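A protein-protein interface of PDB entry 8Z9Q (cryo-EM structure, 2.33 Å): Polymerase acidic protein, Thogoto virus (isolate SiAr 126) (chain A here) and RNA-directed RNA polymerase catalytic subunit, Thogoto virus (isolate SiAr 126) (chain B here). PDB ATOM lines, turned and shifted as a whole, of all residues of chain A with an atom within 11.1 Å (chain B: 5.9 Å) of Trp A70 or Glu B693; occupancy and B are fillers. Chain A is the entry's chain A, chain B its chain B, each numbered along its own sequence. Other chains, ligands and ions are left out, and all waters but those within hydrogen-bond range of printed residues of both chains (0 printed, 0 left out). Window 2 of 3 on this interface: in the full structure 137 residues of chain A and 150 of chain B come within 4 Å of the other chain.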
ATOM      1  N   ASP A  58      -8.148 -26.665 -16.995  1.00  0.00           N
ATOM      2  CA  ASP A  58      -8.551 -27.502 -15.872  1.00  0.00           C
ATOM      3  C   ASP A  58     -10.005 -27.900 -16.070  1.00  0.00           C
ATOM      4  O   ASP A  58     -10.885 -27.034 -16.114  1.00  0.00           O
ATOM      5  CB  ASP A  58      -8.369 -26.768 -14.541  1.00  0.00           C
ATOM      6  CG  ASP A  58      -6.929 -26.374 -14.283  1.00  0.00           C
ATOM      7  OD1 ASP A  58      -6.106 -27.271 -14.010  1.00  0.00           O
ATOM      8  OD2 ASP A  58      -6.621 -25.166 -14.350  1.00  0.00           O
ATOM      9  N   PHE A  60     -12.944 -28.853 -14.634  1.00  0.00           N
ATOM     10  CA  PHE A  60     -13.632 -28.918 -13.349  1.00  0.00           C
ATOM     11  C   PHE A  60     -14.874 -29.796 -13.390  1.00  0.00           C
ATOM     12  O   PHE A  60     -15.317 -30.269 -12.339  1.00  0.00           O
ATOM     13  CB  PHE A  60     -14.021 -27.514 -12.883  1.00  0.00           C
ATOM     14  CG  PHE A  60     -12.859 -26.674 -12.443  1.00  0.00           C
ATOM     15  CD1 PHE A  60     -11.645 -27.256 -12.126  1.00  0.00           C
ATOM     16  CD2 PHE A  60     -12.983 -25.298 -12.345  1.00  0.00           C
ATOM     17  CE1 PHE A  60     -10.576 -26.483 -11.718  1.00  0.00           C
ATOM     18  CE2 PHE A  60     -11.919 -24.520 -11.939  1.00  0.00           C
ATOM     19  CZ  PHE A  60     -10.714 -25.113 -11.625  1.00  0.00           C
ATOM     20  N   GLN A  63     -15.562 -33.476 -11.502  1.00  0.00           N
ATOM     21  CA  GLN A  63     -14.313 -33.645 -10.780  1.00  0.00           C
ATOM     22  C   GLN A  63     -14.589 -33.486  -9.291  1.00  0.00           C
ATOM     23  O   GLN A  63     -15.562 -32.836  -8.895  1.00  0.00           O
ATOM     24  CB  GLN A  63     -13.261 -32.631 -11.258  1.00  0.00           C
ATOM     25  CG  GLN A  63     -11.883 -32.782 -10.637  1.00  0.00           C
ATOM     26  CD  GLN A  63     -10.886 -31.788 -11.196  1.00  0.00           C
ATOM     27  OE1 GLN A  63     -11.228 -30.950 -12.025  1.00  0.00           O
ATOM     28  NE2 GLN A  63      -9.636 -31.906 -10.775  1.00  0.00           N
ATOM     29  N   ASP A  64     -13.738 -34.104  -8.471  1.00  0.00           N
ATOM     30  CA  ASP A  64     -13.924 -34.079  -7.025  1.00  0.00           C
ATOM     31  C   ASP A  64     -14.003 -32.633  -6.554  1.00  0.00           C
ATOM     32  O   ASP A  64     -13.180 -31.796  -6.933  1.00  0.00           O
ATOM     33  CB  ASP A  64     -12.767 -34.824  -6.345  1.00  0.00           C
ATOM     34  CG  ASP A  64     -12.695 -34.604  -4.828  1.00  0.00           C
ATOM     35  OD1 ASP A  64     -13.569 -33.940  -4.232  1.00  0.00           O
ATOM     36  OD2 ASP A  64     -11.730 -35.108  -4.219  1.00  0.00           O
ATOM     37  N   ARG A  65     -15.007 -32.343  -5.721  1.00  0.00           N
ATOM     38  CA  ARG A  65     -15.241 -30.969  -5.292  1.00  0.00           C
ATOM     39  C   ARG A  65     -14.101 -30.459  -4.418  1.00  0.00           C
ATOM     40  O   ARG A  65     -13.735 -29.281  -4.495  1.00  0.00           O
ATOM     41  CB  ARG A  65     -16.582 -30.873  -4.562  1.00  0.00           C
ATOM     42  CG  ARG A  65     -16.775 -29.607  -3.742  1.00  0.00           C
ATOM     43  CD  ARG A  65     -16.759 -28.365  -4.621  1.00  0.00           C
ATOM     44  NE  ARG A  65     -17.703 -28.458  -5.726  1.00  0.00           N
ATOM     45  CZ  ARG A  65     -17.920 -27.492  -6.608  1.00  0.00           C
ATOM     46  NH1 ARG A  65     -17.277 -26.338  -6.541  1.00  0.00           N
ATOM     47  NH2 ARG A  65     -18.803 -27.690  -7.584  1.00  0.00           N
ATOM     48  N   SER A  66     -13.528 -31.325  -3.580  1.00  0.00           N
ATOM     49  CA  SER A  66     -12.384 -30.914  -2.770  1.00  0.00           C
ATOM     50  C   SER A  66     -11.202 -30.532  -3.651  1.00  0.00           C
ATOM     51  O   SER A  66     -10.493 -29.558  -3.368  1.00  0.00           O
ATOM     52  CB  SER A  66     -11.997 -32.033  -1.803  1.00  0.00           C
ATOM     53  OG  SER A  66     -13.040 -32.298  -0.883  1.00  0.00           O
ATOM     54  N   THR A  67     -10.975 -31.287  -4.727  1.00  0.00           N
ATOM     55  CA  THR A  67      -9.932 -30.927  -5.681  1.00  0.00           C
ATOM     56  C   THR A  67     -10.228 -29.588  -6.344  1.00  0.00           C
ATOM     57  O   THR A  67      -9.321 -28.769  -6.539  1.00  0.00           O
ATOM     58  CB  THR A  67      -9.789 -32.020  -6.736  1.00  0.00           C
ATOM     59  OG1 THR A  67      -9.400 -33.248  -6.108  1.00  0.00           O
ATOM     60  CG2 THR A  67      -8.752 -31.622  -7.763  1.00  0.00           C
ATOM     61  N   ILE A  68     -11.490 -29.354  -6.706  1.00  0.00           N
ATOM     62  CA  ILE A  68     -11.869 -28.078  -7.305  1.00  0.00           C
ATOM     63  C   ILE A  68     -11.581 -26.938  -6.340  1.00  0.00           C
ATOM     64  O   ILE A  68     -11.058 -25.889  -6.732  1.00  0.00           O
ATOM     65  CB  ILE A  68     -13.352 -28.104  -7.722  1.00  0.00           C
ATOM     66  CG1 ILE A  68     -13.548 -28.996  -8.946  1.00  0.00           C
ATOM     67  CG2 ILE A  68     -13.856 -26.698  -8.006  1.00  0.00           C
ATOM     68  CD1 ILE A  68     -14.984 -29.083  -9.400  1.00  0.00           C
ATOM     69  N   GLU A  69     -11.911 -27.129  -5.062  1.00  0.00           N
ATOM     70  CA  GLU A  69     -11.662 -26.093  -4.068  1.00  0.00           C
ATOM     71  C   GLU A  69     -10.172 -25.873  -3.843  1.00  0.00           C
ATOM     72  O   GLU A  69      -9.752 -24.741  -3.604  1.00  0.00           O
ATOM     73  CB  GLU A  69     -12.359 -26.445  -2.756  1.00  0.00           C
ATOM     74  CG  GLU A  69     -13.874 -26.513  -2.867  1.00  0.00           C
ATOM     75  CD  GLU A  69     -14.515 -25.153  -3.077  1.00  0.00           C
ATOM     76  OE1 GLU A  69     -13.828 -24.127  -2.885  1.00  0.00           O
ATOM     77  OE2 GLU A  69     -15.709 -25.109  -3.439  1.00  0.00           O
ATOM     78  N   TRP A  70      -9.362 -26.930  -3.912  1.00  0.00           N
ATOM     79  CA  TRP A  70      -7.913 -26.759  -3.826  1.00  0.00           C
ATOM     80  C   TRP A  70      -7.386 -25.934  -4.996  1.00  0.00           C
ATOM     81  O   TRP A  70      -6.621 -24.974  -4.812  1.00  0.00           O
ATOM     82  CB  TRP A  70      -7.235 -28.130  -3.779  1.00  0.00           C
ATOM     83  CG  TRP A  70      -5.731 -28.101  -3.857  1.00  0.00           C
ATOM     84  CD1 TRP A  70      -4.947 -28.839  -4.694  1.00  0.00           C
ATOM     85  CD2 TRP A  70      -4.834 -27.319  -3.053  1.00  0.00           C
ATOM     86  NE1 TRP A  70      -3.621 -28.557  -4.475  1.00  0.00           N
ATOM     87  CE2 TRP A  70      -3.524 -27.628  -3.474  1.00  0.00           C
ATOM     88  CE3 TRP A  70      -5.008 -26.387  -2.026  1.00  0.00           C
ATOM     89  CZ2 TRP A  70      -2.399 -27.037  -2.904  1.00  0.00           C
ATOM     90  CZ3 TRP A  70      -3.890 -25.798  -1.465  1.00  0.00           C
ATOM     91  CH2 TRP A  70      -2.602 -26.128  -1.902  1.00  0.00           C
ATOM     92  N   ILE A  71      -7.801 -26.290  -6.216  1.00  0.00           N
ATOM     93  CA  ILE A  71      -7.348 -25.570  -7.402  1.00  0.00           C
ATOM     94  C   ILE A  71      -7.822 -24.123  -7.373  1.00  0.00           C
ATOM     95  O   ILE A  71      -7.127 -23.226  -7.862  1.00  0.00           O
ATOM     96  CB  ILE A  71      -7.812 -26.296  -8.680  1.00  0.00           C
ATOM     97  CG1 ILE A  71      -7.299 -27.737  -8.688  1.00  0.00           C
ATOM     98  CG2 ILE A  71      -7.333 -25.563  -9.924  1.00  0.00           C
ATOM     99  CD1 ILE A  71      -7.482 -28.448 -10.011  1.00  0.00           C
ATOM    100  N   CYS A  72      -9.006 -23.871  -6.811  1.00  0.00           N
ATOM    101  CA  CYS A  72      -9.495 -22.503  -6.679  1.00  0.00           C
ATOM    102  C   CYS A  72      -8.807 -21.751  -5.544  1.00  0.00           C
ATOM    103  O   CYS A  72      -8.690 -20.523  -5.605  1.00  0.00           O
ATOM    104  CB  CYS A  72     -11.010 -22.503  -6.473  1.00  0.00           C
ATOM    105  SG  CYS A  72     -11.949 -23.086  -7.903  1.00  0.00           S
ATOM    106  N   SER A  73      -8.362 -22.457  -4.503  1.00  0.00           N
ATOM    107  CA  SER A  73      -7.532 -21.826  -3.486  1.00  0.00           C
ATOM    108  C   SER A  73      -6.227 -21.342  -4.093  1.00  0.00           C
ATOM    109  O   SER A  73      -5.766 -20.233  -3.798  1.00  0.00           O
ATOM    110  CB  SER A  73      -7.268 -22.800  -2.340  1.00  0.00           C
ATOM    111  OG  SER A  73      -6.307 -23.766  -2.721  1.00  0.00           O
ATOM    112  N   LYS A  74      -5.616 -22.160  -4.947  1.00  0.00           N
ATOM    113  CA  LYS A  74      -4.609 -21.613  -5.841  1.00  0.00           C
ATOM    114  C   LYS A  74      -5.290 -20.741  -6.892  1.00  0.00           C
ATOM    115  O   LYS A  74      -6.506 -20.798  -7.084  1.00  0.00           O
ATOM    116  CB  LYS A  74      -3.800 -22.728  -6.504  1.00  0.00           C
ATOM    117  CG  LYS A  74      -3.059 -23.620  -5.524  1.00  0.00           C
ATOM    118  CD  LYS A  74      -3.240 -25.089  -5.861  1.00  0.00           C
ATOM    119  CE  LYS A  74      -2.694 -25.406  -7.242  1.00  0.00           C
ATOM    120  NZ  LYS A  74      -2.657 -26.872  -7.502  1.00  0.00           N
ATOM    121  N   LYS A  75      -4.502 -19.871  -7.526  1.00  0.00           N
ATOM    122  CA  LYS A  75      -4.980 -19.033  -8.626  1.00  0.00           C
ATOM    123  C   LYS A  75      -5.928 -17.946  -8.120  1.00  0.00           C
ATOM    124  O   LYS A  75      -6.338 -17.070  -8.888  1.00  0.00           O
ATOM    125  CB  LYS A  75      -5.674 -19.886  -9.693  1.00  0.00           C
ATOM    126  CG  LYS A  75      -4.760 -20.863 -10.406  1.00  0.00           C
ATOM    127  CD  LYS A  75      -5.526 -21.678 -11.431  1.00  0.00           C
ATOM    128  CE  LYS A  75      -4.624 -22.693 -12.111  1.00  0.00           C
ATOM    129  NZ  LYS A  75      -5.365 -23.519 -13.104  1.00  0.00           N
ATOM    130  N   LYS A  76      -6.274 -17.999  -6.834  1.00  0.00           N
ATOM    131  CA  LYS A  76      -7.104 -16.996  -6.160  1.00  0.00           C
ATOM    132  C   LYS A  76      -8.439 -16.781  -6.877  1.00  0.00           C
ATOM    133  O   LYS A  76      -8.746 -15.695  -7.372  1.00  0.00           O
ATOM    134  CB  LYS A  76      -6.344 -15.674  -6.002  1.00  0.00           C
ATOM    135  CG  LYS A  76      -4.854 -15.826  -5.714  1.00  0.00           C
ATOM    136  CD  LYS A  76      -4.608 -16.647  -4.456  1.00  0.00           C
ATOM    137  CE  LYS A  76      -3.158 -17.092  -4.362  1.00  0.00           C
ATOM    138  NZ  LYS A  76      -2.929 -17.989  -3.195  1.00  0.00           N
ATOM    139  N   VAL A  77      -9.240 -17.848  -6.923  1.00  0.00           N
ATOM    140  CA  VAL A  77     -10.596 -17.796  -7.458  1.00  0.00           C
ATOM    141  C   VAL A  77     -11.520 -18.574  -6.530  1.00  0.00           C
ATOM    142  O   VAL A  77     -11.078 -19.355  -5.685  1.00  0.00           O
ATOM    143  CB  VAL A  77     -10.695 -18.351  -8.898  1.00  0.00           C
ATOM    144  CG1 VAL A  77      -9.864 -17.513  -9.859  1.00  0.00           C
ATOM    145  CG2 VAL A  77     -10.256 -19.802  -8.941  1.00  0.00           C
ATOM    146  N   GLN A  78     -12.821 -18.345  -6.688  1.00  0.00           N
ATOM    147  CA  GLN A  78     -13.815 -19.043  -5.883  1.00  0.00           C
ATOM    148  C   GLN A  78     -15.102 -19.169  -6.684  1.00  0.00           C
ATOM    149  O   GLN A  78     -15.616 -18.168  -7.191  1.00  0.00           O
ATOM    150  CB  GLN A  78     -14.074 -18.308  -4.563  1.00  0.00           C
ATOM    151  CG  GLN A  78     -15.044 -19.018  -3.632  1.00  0.00           C
ATOM    152  CD  GLN A  78     -14.452 -20.264  -2.998  1.00  0.00           C
ATOM    153  OE1 GLN A  78     -14.266 -21.286  -3.657  1.00  0.00           O
ATOM    154  NE2 GLN A  78     -14.155 -20.182  -1.707  1.00  0.00           N
ATOM    155  N   TYR A  79     -15.618 -20.393  -6.788  1.00  0.00           N
ATOM    156  CA  TYR A  79     -16.784 -20.672  -7.611  1.00  0.00           C
ATOM    157  C   TYR A  79     -17.833 -21.410  -6.787  1.00  0.00           C
ATOM    158  O   TYR A  79     -17.513 -22.424  -6.142  1.00  0.00           O
ATOM    159  CB  TYR A  79     -16.391 -21.501  -8.840  1.00  0.00           C
ATOM    160  CG  TYR A  79     -15.539 -20.745  -9.831  1.00  0.00           C
ATOM    161  CD1 TYR A  79     -14.342 -21.273 -10.290  1.00  0.00           C
ATOM    162  CD2 TYR A  79     -15.927 -19.497 -10.297  1.00  0.00           C
ATOM    163  CE1 TYR A  79     -13.557 -20.583 -11.192  1.00  0.00           C
ATOM    164  CE2 TYR A  79     -15.149 -18.800 -11.199  1.00  0.00           C
ATOM    165  CZ  TYR A  79     -13.965 -19.347 -11.642  1.00  0.00           C
ATOM    166  OH  TYR A  79     -13.188 -18.655 -12.540  1.00  0.00           O
ATOM    167  N   THR A  84     -20.585 -23.863 -11.002  1.00  0.00           N
ATOM    168  CA  THR A  84     -19.158 -24.088 -11.201  1.00  0.00           C
ATOM    169  C   THR A  84     -18.842 -24.180 -12.690  1.00  0.00           C
ATOM    170  O   THR A  84     -19.445 -24.994 -13.395  1.00  0.00           O
ATOM    171  CB  THR A  84     -18.709 -25.364 -10.497  1.00  0.00           C
ATOM    172  OG1 THR A  84     -18.947 -25.245  -9.089  1.00  0.00           O
ATOM    173  CG2 THR A  84     -17.227 -25.610 -10.737  1.00  0.00           C
ATOM    174  N   TYR A  88     -11.212 -23.909 -16.992  1.00  0.00           N
ATOM    175  CA  TYR A  88     -10.477 -22.705 -16.626  1.00  0.00           C
ATOM    176  C   TYR A  88      -9.254 -22.609 -17.524  1.00  0.00           C
ATOM    177  O   TYR A  88      -8.522 -23.590 -17.680  1.00  0.00           O
ATOM    178  CB  TYR A  88     -10.068 -22.726 -15.146  1.00  0.00           C
ATOM    179  CG  TYR A  88      -9.384 -21.463 -14.657  1.00  0.00           C
ATOM    180  CD1 TYR A  88      -8.045 -21.215 -14.934  1.00  0.00           C
ATOM    181  CD2 TYR A  88     -10.082 -20.520 -13.916  1.00  0.00           C
ATOM    182  CE1 TYR A  88      -7.425 -20.065 -14.490  1.00  0.00           C
ATOM    183  CE2 TYR A  88      -9.470 -19.367 -13.467  1.00  0.00           C
ATOM    184  CZ  TYR A  88      -8.142 -19.144 -13.756  1.00  0.00           C
ATOM    185  OH  TYR A  88      -7.529 -17.996 -13.310  1.00  0.00           O
ATOM    186  N   ARG B 686      -8.673 -40.196  -4.693  1.00  0.00           N
ATOM    187  CA  ARG B 686      -8.409 -38.798  -4.996  1.00  0.00           C
ATOM    188  C   ARG B 686      -8.247 -37.984  -3.718  1.00  0.00           C
ATOM    189  O   ARG B 686      -7.445 -37.043  -3.677  1.00  0.00           O
ATOM    190  CB  ARG B 686      -9.510 -38.201  -5.872  1.00  0.00           C
ATOM    191  CG  ARG B 686      -9.216 -36.744  -6.167  1.00  0.00           C
ATOM    192  CD  ARG B 686      -7.951 -36.719  -7.021  1.00  0.00           C
ATOM    193  NE  ARG B 686      -7.505 -35.394  -7.431  1.00  0.00           N
ATOM    194  CZ  ARG B 686      -6.718 -34.623  -6.691  1.00  0.00           C
ATOM    195  NH1 ARG B 686      -6.324 -34.996  -5.486  1.00  0.00           N
ATOM    196  NH2 ARG B 686      -6.297 -33.462  -7.182  1.00  0.00           N
ATOM    197  N   LEU B 688      -6.917 -39.098  -0.924  1.00  0.00           N
ATOM    198  CA  LEU B 688      -5.559 -39.394  -0.483  1.00  0.00           C
ATOM    199  C   LEU B 688      -4.534 -38.658  -1.337  1.00  0.00           C
ATOM    200  O   LEU B 688      -3.549 -38.122  -0.815  1.00  0.00           O
ATOM    201  CB  LEU B 688      -5.319 -40.903  -0.519  1.00  0.00           C
ATOM    202  CG  LEU B 688      -3.978 -41.419   0.001  1.00  0.00           C
ATOM    203  CD1 LEU B 688      -3.808 -41.078   1.470  1.00  0.00           C
ATOM    204  CD2 LEU B 688      -3.886 -42.918  -0.212  1.00  0.00           C
ATOM    205  N   GLU B 689      -4.757 -38.607  -2.653  1.00  0.00           N
ATOM    206  CA  GLU B 689      -3.865 -37.836  -3.514  1.00  0.00           C
ATOM    207  C   GLU B 689      -3.840 -36.370  -3.105  1.00  0.00           C
ATOM    208  O   GLU B 689      -2.773 -35.749  -3.058  1.00  0.00           O
ATOM    209  CB  GLU B 689      -4.288 -37.967  -4.976  1.00  0.00           C
ATOM    210  CG  GLU B 689      -4.006 -39.319  -5.599  1.00  0.00           C
ATOM    211  CD  GLU B 689      -4.718 -39.498  -6.923  1.00  0.00           C
ATOM    212  OE1 GLU B 689      -5.200 -38.489  -7.479  1.00  0.00           O
ATOM    213  OE2 GLU B 689      -4.797 -40.644  -7.410  1.00  0.00           O
ATOM    214  N   LEU B 690      -5.008 -35.801  -2.804  1.00  0.00           N
ATOM    215  CA  LEU B 690      -5.080 -34.396  -2.417  1.00  0.00           C
ATOM    216  C   LEU B 690      -4.371 -34.143  -1.091  1.00  0.00           C
ATOM    217  O   LEU B 690      -3.643 -33.153  -0.952  1.00  0.00           O
ATOM    218  CB  LEU B 690      -6.540 -33.953  -2.341  1.00  0.00           C
ATOM    219  CG  LEU B 690      -6.812 -32.572  -1.748  1.00  0.00           C
ATOM    220  CD1 LEU B 690      -6.395 -31.492  -2.727  1.00  0.00           C
ATOM    221  CD2 LEU B 690      -8.279 -32.428  -1.385  1.00  0.00           C
ATOM    222  N   VAL B 691      -4.572 -35.022  -0.105  1.00  0.00           N
ATOM    223  CA  VAL B 691      -3.947 -34.796   1.195  1.00  0.00           C
ATOM    224  C   VAL B 691      -2.436 -34.982   1.105  1.00  0.00           C
ATOM    225  O   VAL B 691      -1.682 -34.323   1.831  1.00  0.00           O
ATOM    226  CB  VAL B 691      -4.578 -35.693   2.279  1.00  0.00           C
ATOM    227  CG1 VAL B 691      -4.264 -37.154   2.042  1.00  0.00           C
ATOM    228  CG2 VAL B 691      -4.119 -35.260   3.664  1.00  0.00           C
ATOM    229  N   VAL B 692      -1.961 -35.868   0.225  1.00  0.00           N
ATOM    230  CA  VAL B 692      -0.521 -35.973   0.010  1.00  0.00           C
ATOM    231  C   VAL B 692       0.009 -34.736  -0.705  1.00  0.00           C
ATOM    232  O   VAL B 692       1.071 -34.207  -0.356  1.00  0.00           O
ATOM    233  CB  VAL B 692      -0.178 -37.262  -0.760  1.00  0.00           C
ATOM    234  CG1 VAL B 692       1.307 -37.304  -1.072  1.00  0.00           C
ATOM    235  CG2 VAL B 692      -0.567 -38.479   0.054  1.00  0.00           C
ATOM    236  N   GLU B 693      -0.722 -34.251  -1.712  1.00  0.00           N
ATOM    237  CA  GLU B 693      -0.260 -33.107  -2.489  1.00  0.00           C
ATOM    238  C   GLU B 693      -0.232 -31.832  -1.657  1.00  0.00           C
ATOM    239  O   GLU B 693       0.603 -30.954  -1.903  1.00  0.00           O
ATOM    240  CB  GLU B 693      -1.146 -32.931  -3.725  1.00  0.00           C
ATOM    241  CG  GLU B 693      -0.644 -31.923  -4.751  1.00  0.00           C
ATOM    242  CD  GLU B 693      -1.026 -30.495  -4.415  1.00  0.00           C
ATOM    243  OE1 GLU B 693      -2.071 -30.298  -3.759  1.00  0.00           O
ATOM    244  OE2 GLU B 693      -0.283 -29.571  -4.807  1.00  0.00           O
ATOM    245  N   ARG B 694      -1.123 -31.709  -0.677  1.00  0.00           N
ATOM    246  CA  ARG B 694      -1.192 -30.516   0.162  1.00  0.00           C
ATOM    247  C   ARG B 694      -0.604 -30.788   1.548  1.00  0.00           C
ATOM    248  O   ARG B 694      -1.108 -30.331   2.577  1.00  0.00           O
ATOM    249  CB  ARG B 694      -2.638 -30.019   0.228  1.00  0.00           C
ATOM    250  CG  ARG B 694      -2.879 -28.718   0.981  1.00  0.00           C
ATOM    251  CD  ARG B 694      -4.333 -28.302   0.885  1.00  0.00           C
ATOM    252  NE  ARG B 694      -4.601 -27.074   1.624  1.00  0.00           N
ATOM    253  CZ  ARG B 694      -5.786 -26.485   1.685  1.00  0.00           C
ATOM    254  NH1 ARG B 694      -6.824 -26.950   1.009  1.00  0.00           N
ATOM    255  NH2 ARG B 694      -5.930 -25.391   2.427  1.00  0.00           N
ATOM    256  N   SER B 695       0.477 -31.562   1.593  1.00  0.00           N
ATOM    257  CA  SER B 695       1.161 -31.898   2.834  1.00  0.00           C
ATOM    258  C   SER B 695       2.428 -31.081   3.050  1.00  0.00           C
ATOM    259  O   SER B 695       3.224 -31.421   3.931  1.00  0.00           O
ATOM    260  CB  SER B 695       1.491 -33.391   2.865  1.00  0.00           C
ATOM    261  OG  SER B 695       2.433 -33.724   1.861  1.00  0.00           O
ATOM    262  N   ASP B 696       2.626 -30.019   2.264  1.00  0.00           N
ATOM    263  CA  ASP B 696       3.790 -29.132   2.318  1.00  0.00           C
ATOM    264  C   ASP B 696       5.105 -29.885   2.496  1.00  0.00           C
ATOM    265  O   ASP B 696       5.981 -29.450   3.251  1.00  0.00           O
ATOM    266  CB  ASP B 696       3.618 -28.074   3.421  1.00  0.00           C
ATOM    267  CG  ASP B 696       3.471 -28.674   4.808  1.00  0.00           C
ATOM    268  OD1 ASP B 696       4.500 -28.914   5.474  1.00  0.00           O
ATOM    269  OD2 ASP B 696       2.321 -28.901   5.237  1.00  0.00           O
ATOM    270  N   LYS B 702       6.715 -36.519  -2.168  1.00  0.00           N
ATOM    271  CA  LYS B 702       5.335 -36.590  -2.636  1.00  0.00           C
ATOM    272  C   LYS B 702       5.201 -37.560  -3.803  1.00  0.00           C
ATOM    273  O   LYS B 702       4.276 -38.380  -3.843  1.00  0.00           O
ATOM    274  CB  LYS B 702       4.850 -35.196  -3.035  1.00  0.00           C
ATOM    275  CG  LYS B 702       4.580 -34.275  -1.860  1.00  0.00           C
ATOM    276  CD  LYS B 702       3.875 -33.007  -2.305  1.00  0.00           C
ATOM    277  CE  LYS B 702       3.609 -32.084  -1.129  1.00  0.00           C
ATOM    278  NZ  LYS B 702       2.877 -30.856  -1.542  1.00  0.00           N
ATOM    279  N   LEU B 706       2.976 -41.001  -3.857  1.00  0.00           N
ATOM    280  CA  LEU B 706       1.928 -41.257  -4.843  1.00  0.00           C
ATOM    281  C   LEU B 706       2.258 -42.449  -5.733  1.00  0.00           C
ATOM    282  O   LEU B 706       1.346 -43.076  -6.283  1.00  0.00           O
ATOM    283  CB  LEU B 706       1.671 -40.017  -5.699  1.00  0.00           C
ATOM    284  CG  LEU B 706       1.426 -38.689  -4.985  1.00  0.00           C
ATOM    285  CD1 LEU B 706       1.435 -37.539  -5.979  1.00  0.00           C
ATOM    286  CD2 LEU B 706       0.110 -38.732  -4.229  1.00  0.00           C
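NE1 of Trp A70 lies within hydrogen-bond range of OE1 of Glu B693 (2.4 Å). The side-chain hydroxyl of Thr A67 lies close to the guanidinium group of Arg B686 (3.2 Å).
The side-chain hydroxyl (OG) of Ser A73 is in hydrogen-bond range of the backbone carbonyl oxygen (O) of Trp A70 (2.4 Å). The backbone NH (N) of Ser A66 is in hydrogen-bond range of the side-chain carboxylate (OD1) of Asp A64, at 2.7 Å. OE1 of Glu B689 is in salt-bridge range of NE of Arg B686 (3.9 Å).
Asp A64 touches Arg B686 (OD2 to CG, 3.6 Å). CD2 of Leu B690 touches CB of Ser A66, at 3.8 Å. Trp A70 touches Leu B690. NE of Arg B694 touches CZ3 of Trp A70 (3.4 Å).
Of the printed residues of chain B, Asp A64 touches Arg B686 (3.6 Å). Printed residues of chain B within 4 Å of Ser A66: Leu B690 (3.8 Å). Printed residues of chain B within 4 Å of Thr A67: Arg B686. Ile A68 touches none of the printed residues of chain B. Of the printed residues of chain A, Arg B686 touches Asp A64 and Thr A67. Glu B689 touches none of the printed residues of chain A. Leu B690 touches just these residues of chain A: Ser A66 and Trp A70. No residue of chain A comes within 4 Å of Val B691. No residue of chain A comes within 4 Å of Val B692. Of the printed residues of chain A, Glu B693 touches Trp A70. No residue of chain A comes within 4 Å of Ser B695. The nearest printed residue of chain B that does not touch Ser A66 is Arg B694 (6.3 Å).
Printed residues of chain A that touch a printed residue of chain B: Asp A64, Ser A66, Thr A67 and Trp A70. Printed residues of chain B that touch a printed residue of chain A: Arg B686, Leu B690, Glu B693 and Arg B694.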
